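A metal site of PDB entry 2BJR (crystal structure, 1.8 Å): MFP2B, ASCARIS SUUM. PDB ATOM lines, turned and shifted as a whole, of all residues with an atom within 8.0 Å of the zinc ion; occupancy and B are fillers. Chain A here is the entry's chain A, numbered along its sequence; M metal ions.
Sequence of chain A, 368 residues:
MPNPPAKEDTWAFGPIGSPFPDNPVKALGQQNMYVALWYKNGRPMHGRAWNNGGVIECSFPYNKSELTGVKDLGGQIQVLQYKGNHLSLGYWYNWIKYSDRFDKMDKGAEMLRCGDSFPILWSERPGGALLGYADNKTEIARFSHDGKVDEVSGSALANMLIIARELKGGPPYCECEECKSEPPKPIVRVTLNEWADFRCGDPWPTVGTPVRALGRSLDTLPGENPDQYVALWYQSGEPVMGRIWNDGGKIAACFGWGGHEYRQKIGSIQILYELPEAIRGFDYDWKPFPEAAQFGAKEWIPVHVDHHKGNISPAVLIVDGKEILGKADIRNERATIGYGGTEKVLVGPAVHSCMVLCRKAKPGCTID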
ATOM      1  N   ASN A  85      17.799  12.271   8.162  1.00  0.00           N
ATOM      2  CA  ASN A  85      17.901  11.588   9.431  1.00  0.00           C
ATOM      3  C   ASN A  85      18.120  10.099   9.240  1.00  0.00           C
ATOM      4  O   ASN A  85      18.275   9.614   8.105  1.00  0.00           O
ATOM      5  CB  ASN A  85      16.701  11.918  10.333  1.00  0.00           C
ATOM      6  CG  ASN A  85      15.383  11.390   9.783  1.00  0.00           C
ATOM      7  OD1 ASN A  85      15.345  10.412   9.024  1.00  0.00           O
ATOM      8  ND2 ASN A  85      14.287  12.061  10.169  1.00  0.00           N
ATOM      9  N   HIS A  86      18.172   9.361  10.332  1.00  0.00           N
ATOM     10  CA  HIS A  86      18.538   7.956  10.248  1.00  0.00           C
ATOM     11  C   HIS A  86      17.562   7.094   9.425  1.00  0.00           C
ATOM     12  O   HIS A  86      17.942   6.037   8.957  1.00  0.00           O
ATOM     13  CB  HIS A  86      18.728   7.359  11.629  1.00  0.00           C
ATOM     14  CG  HIS A  86      17.465   7.345  12.436  1.00  0.00           C
ATOM     15  ND1 HIS A  86      16.658   6.229  12.521  1.00  0.00           N
ATOM     16  CD2 HIS A  86      16.868   8.307  13.182  1.00  0.00           C
ATOM     17  CE1 HIS A  86      15.631   6.496  13.308  1.00  0.00           C
ATOM     18  NE2 HIS A  86      15.719   7.750  13.692  1.00  0.00           N
ATOM     19  N   LEU A  87      16.320   7.530   9.245  1.00  0.00           N
ATOM     20  CA  LEU A  87      15.382   6.789   8.397  1.00  0.00           C
ATOM     21  C   LEU A  87      15.810   6.753   6.937  1.00  0.00           C
ATOM     22  O   LEU A  87      15.707   5.718   6.305  1.00  0.00           O
ATOM     23  CB  LEU A  87      13.985   7.393   8.468  1.00  0.00           C
ATOM     24  CG  LEU A  87      13.331   7.417   9.857  1.00  0.00           C
ATOM     25  CD1 LEU A  87      11.897   7.974   9.716  1.00  0.00           C
ATOM     26  CD2 LEU A  87      13.375   6.052  10.510  1.00  0.00           C
ATOM     27  N   TRP A  92      23.368   7.630  12.235  1.00  0.00           N
ATOM     28  CA  TRP A  92      23.524   8.953  12.878  1.00  0.00           C
ATOM     29  C   TRP A  92      24.897   8.987  13.543  1.00  0.00           C
ATOM     30  O   TRP A  92      25.506   7.946  13.808  1.00  0.00           O
ATOM     31  CB  TRP A  92      22.432   9.231  13.931  1.00  0.00           C
ATOM     32  CG  TRP A  92      22.231   8.158  14.995  1.00  0.00           C
ATOM     33  CD1 TRP A  92      21.533   6.973  14.868  1.00  0.00           C
ATOM     34  CD2 TRP A  92      22.660   8.198  16.361  1.00  0.00           C
ATOM     35  NE1 TRP A  92      21.548   6.285  16.046  1.00  0.00           N
ATOM     36  CE2 TRP A  92      22.220   7.008  16.989  1.00  0.00           C
ATOM     37  CE3 TRP A  92      23.378   9.116  17.123  1.00  0.00           C
ATOM     38  CZ2 TRP A  92      22.495   6.708  18.320  1.00  0.00           C
ATOM     39  CZ3 TRP A  92      23.624   8.822  18.466  1.00  0.00           C
ATOM     40  CH2 TRP A  92      23.198   7.629  19.038  1.00  0.00           C
ATOM     41  N   GLY A 169      18.695   2.401  15.316  1.00  0.00           N
ATOM     42  CA  GLY A 169      17.888   3.403  15.966  1.00  0.00           C
ATOM     43  C   GLY A 169      18.235   4.815  15.505  1.00  0.00           C
ATOM     44  O   GLY A 169      18.785   5.063  14.422  1.00  0.00           O
ATOM     45  N   GLY A 170      17.874   5.740  16.384  1.00  0.00           N
ATOM     46  CA  GLY A 170      18.056   7.149  16.147  1.00  0.00           C
ATOM     47  C   GLY A 170      18.810   7.758  17.292  1.00  0.00           C
ATOM     48  O   GLY A 170      19.084   7.100  18.318  1.00  0.00           O
ATOM     49  N   PRO A 171      19.166   9.021  17.126  1.00  0.00           N
ATOM     50  CA  PRO A 171      19.871   9.733  18.191  1.00  0.00           C
ATOM     51  C   PRO A 171      18.887  10.011  19.357  1.00  0.00           C
ATOM     52  O   PRO A 171      17.706   9.894  19.153  1.00  0.00           O
ATOM     53  CB  PRO A 171      20.347  11.014  17.508  1.00  0.00           C
ATOM     54  CG  PRO A 171      19.357  11.260  16.412  1.00  0.00           C
ATOM     55  CD  PRO A 171      18.919   9.884  15.954  1.00  0.00           C
ATOM     56  N   PRO A 172      19.418  10.343  20.532  1.00  0.00           N
ATOM     57  CA  PRO A 172      18.621  10.404  21.786  1.00  0.00           C
ATOM     58  C   PRO A 172      17.363  11.297  21.788  1.00  0.00           C
ATOM     59  O   PRO A 172      16.430  10.999  22.574  1.00  0.00           O
ATOM     60  CB  PRO A 172      19.623  10.899  22.839  1.00  0.00           C
ATOM     61  CG  PRO A 172      20.994  10.771  22.227  1.00  0.00           C
ATOM     62  CD  PRO A 172      20.846  10.669  20.746  1.00  0.00           C
ATOM     63  N   TYR A 173      17.324  12.331  20.969  1.00  0.00           N
ATOM     64  CA  TYR A 173      16.192  13.262  20.968  1.00  0.00           C
ATOM     65  C   TYR A 173      15.430  13.231  19.638  1.00  0.00           C
ATOM     66  O   TYR A 173      14.667  14.150  19.319  1.00  0.00           O
ATOM     67  CB  TYR A 173      16.667  14.691  21.277  1.00  0.00           C
ATOM     68  CG  TYR A 173      17.617  14.772  22.465  1.00  0.00           C
ATOM     69  CD1 TYR A 173      18.973  15.072  22.283  1.00  0.00           C
ATOM     70  CD2 TYR A 173      17.162  14.557  23.763  1.00  0.00           C
ATOM     71  CE1 TYR A 173      19.855  15.138  23.359  1.00  0.00           C
ATOM     72  CE2 TYR A 173      18.037  14.626  24.861  1.00  0.00           C
ATOM     73  CZ  TYR A 173      19.379  14.902  24.647  1.00  0.00           C
ATOM     74  OH  TYR A 173      20.249  14.976  25.724  1.00  0.00           O
ATOM     75  N   CYS A 174      15.616  12.182  18.846  1.00  0.00           N
ATOM     76  CA  CYS A 174      14.915  12.091  17.587  1.00  0.00           C
ATOM     77  C   CYS A 174      13.397  12.126  17.763  1.00  0.00           C
ATOM     78  O   CYS A 174      12.873  11.486  18.669  1.00  0.00           O
ATOM     79  CB  CYS A 174      15.285  10.808  16.845  1.00  0.00           C
ATOM     80  SG  CYS A 174      14.777  10.886  15.121  1.00  0.00           S
ATOM     81  N   GLU A 175      12.714  12.833  16.857  1.00  0.00           N
ATOM     82  CA  GLU A 175      11.245  12.964  16.859  1.00  0.00           C
ATOM     83  C   GLU A 175      10.595  12.422  15.576  1.00  0.00           C
ATOM     84  O   GLU A 175       9.453  12.774  15.254  1.00  0.00           O
ATOM     85  CB  GLU A 175      10.839  14.440  17.073  1.00  0.00           C
ATOM     86  CG  GLU A 175      10.241  14.705  18.455  1.00  0.00           C
ATOM     87  CD  GLU A 175      10.456  16.141  18.926  1.00  0.00           C
ATOM     88  OE1 GLU A 175      10.457  17.079  18.087  1.00  0.00           O
ATOM     89  OE2 GLU A 175      10.606  16.318  20.171  1.00  0.00           O
ATOM     90  N   CYS A 176      11.315  11.570  14.847  1.00  0.00           N
ATOM     91  CA  CYS A 176      10.737  10.831  13.724  1.00  0.00           C
ATOM     92  C   CYS A 176       9.694   9.817  14.263  1.00  0.00           C
ATOM     93  O   CYS A 176       9.716   9.449  15.438  1.00  0.00           O
ATOM     94  CB  CYS A 176      11.806  10.109  12.906  1.00  0.00           C
ATOM     95  SG  CYS A 176      12.265   8.474  13.550  1.00  0.00           S
ATOM     96  N   GLU A 177       8.817   9.350  13.398  1.00  0.00           N
ATOM     97  CA  GLU A 177       7.706   8.500  13.839  1.00  0.00           C
ATOM     98  C   GLU A 177       8.128   7.170  14.447  1.00  0.00           C
ATOM     99  O   GLU A 177       7.429   6.662  15.303  1.00  0.00           O
ATOM    100  CB  GLU A 177       6.718   8.245  12.713  1.00  0.00           C
ATOM    101  CG  GLU A 177       5.422   7.606  13.201  1.00  0.00           C
ATOM    102  CD  GLU A 177       4.804   8.339  14.382  1.00  0.00           C
ATOM    103  OE1 GLU A 177       4.188   9.407  14.126  1.00  0.00           O
ATOM    104  OE2 GLU A 177       4.952   7.866  15.550  1.00  0.00           O
ATOM    105  N   GLU A 178       9.263   6.622  14.023  1.00  0.00           N
ATOM    106  CA  GLU A 178       9.754   5.357  14.605  1.00  0.00           C
ATOM    107  C   GLU A 178      10.293   5.538  16.003  1.00  0.00           C
ATOM    108  O   GLU A 178      10.056   4.691  16.869  1.00  0.00           O
ATOM    109  CB  GLU A 178      10.868   4.755  13.742  1.00  0.00           C
ATOM    110  CG  GLU A 178      10.420   4.185  12.398  1.00  0.00           C
ATOM    111  CD  GLU A 178      11.227   2.932  12.042  1.00  0.00           C
ATOM    112  OE1 GLU A 178      11.005   1.883  12.702  1.00  0.00           O
ATOM    113  OE2 GLU A 178      12.100   3.006  11.151  1.00  0.00           O
ATOM    114  N   CYS A 179      11.047   6.630  16.211  1.00  0.00           N
ATOM    115  CA  CYS A 179      11.629   6.915  17.499  1.00  0.00           C
ATOM    116  C   CYS A 179      10.531   7.349  18.485  1.00  0.00           C
ATOM    117  O   CYS A 179      10.568   7.030  19.664  1.00  0.00           O
ATOM    118  CB  CYS A 179      12.714   7.962  17.369  1.00  0.00           C
ATOM    119  SG  CYS A 179      14.167   7.438  16.406  1.00  0.00           S
ATOM    120  N   LYS A 180       9.562   8.103  17.955  1.00  0.00           N
ATOM    121  CA  LYS A 180       8.406   8.537  18.746  1.00  0.00           C
ATOM    122  C   LYS A 180       7.647   7.324  19.296  1.00  0.00           C
ATOM    123  O   LYS A 180       7.218   7.338  20.449  1.00  0.00           O
ATOM    124  CB  LYS A 180       7.458   9.421  17.915  1.00  0.00           C
ATOM    125  CG  LYS A 180       6.863  10.608  18.685  1.00  0.00           C
ATOM    126  CD  LYS A 180       5.733  11.305  17.906  1.00  0.00           C
ATOM    127  CE  LYS A 180       6.260  12.348  16.924  1.00  0.00           C
ATOM    128  NZ  LYS A 180       5.160  12.935  16.096  1.00  0.00           N
ATOM    129  N   GLU A 182       8.868   4.308  19.905  1.00  0.00           N
ATOM    130  CA  GLU A 182       9.680   3.409  20.705  1.00  0.00           C
ATOM    131  C   GLU A 182       9.376   3.674  22.184  1.00  0.00           C
ATOM    132  O   GLU A 182       8.922   4.769  22.537  1.00  0.00           O
ATOM    133  CB  GLU A 182      11.184   3.610  20.432  1.00  0.00           C
ATOM    134  CG  GLU A 182      11.706   2.769  19.272  1.00  0.00           C
ATOM    135  CD  GLU A 182      13.051   3.263  18.726  1.00  0.00           C
ATOM    136  OE1 GLU A 182      13.844   3.870  19.476  1.00  0.00           O
ATOM    137  OE2 GLU A 182      13.311   3.054  17.526  1.00  0.00           O
HETATM  138 ZN    ZN M   1      14.235   8.719  14.716  1.00  0.00          ZN
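SG of Cys 176 lies close to N of Glu 178 (3.6 Å).
The backbone carbonyl oxygen (O) of Gly 169 is in hydrogen-bond range of a ring nitrogen (ND1) of His 86 (3.1 Å).
Of the 17 residues printed, 4 come within 4 Å of the zinc ion.
The zinc ion is bound by a ring nitrogen (NE2) of His 86, the side-chain sulfur (SG) of Cys 179, the side-chain sulfur (SG) of Cys 174 and the side-chain sulfur (SG) of Cys 176.
The zinc ion has four donor atoms within binding distance.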
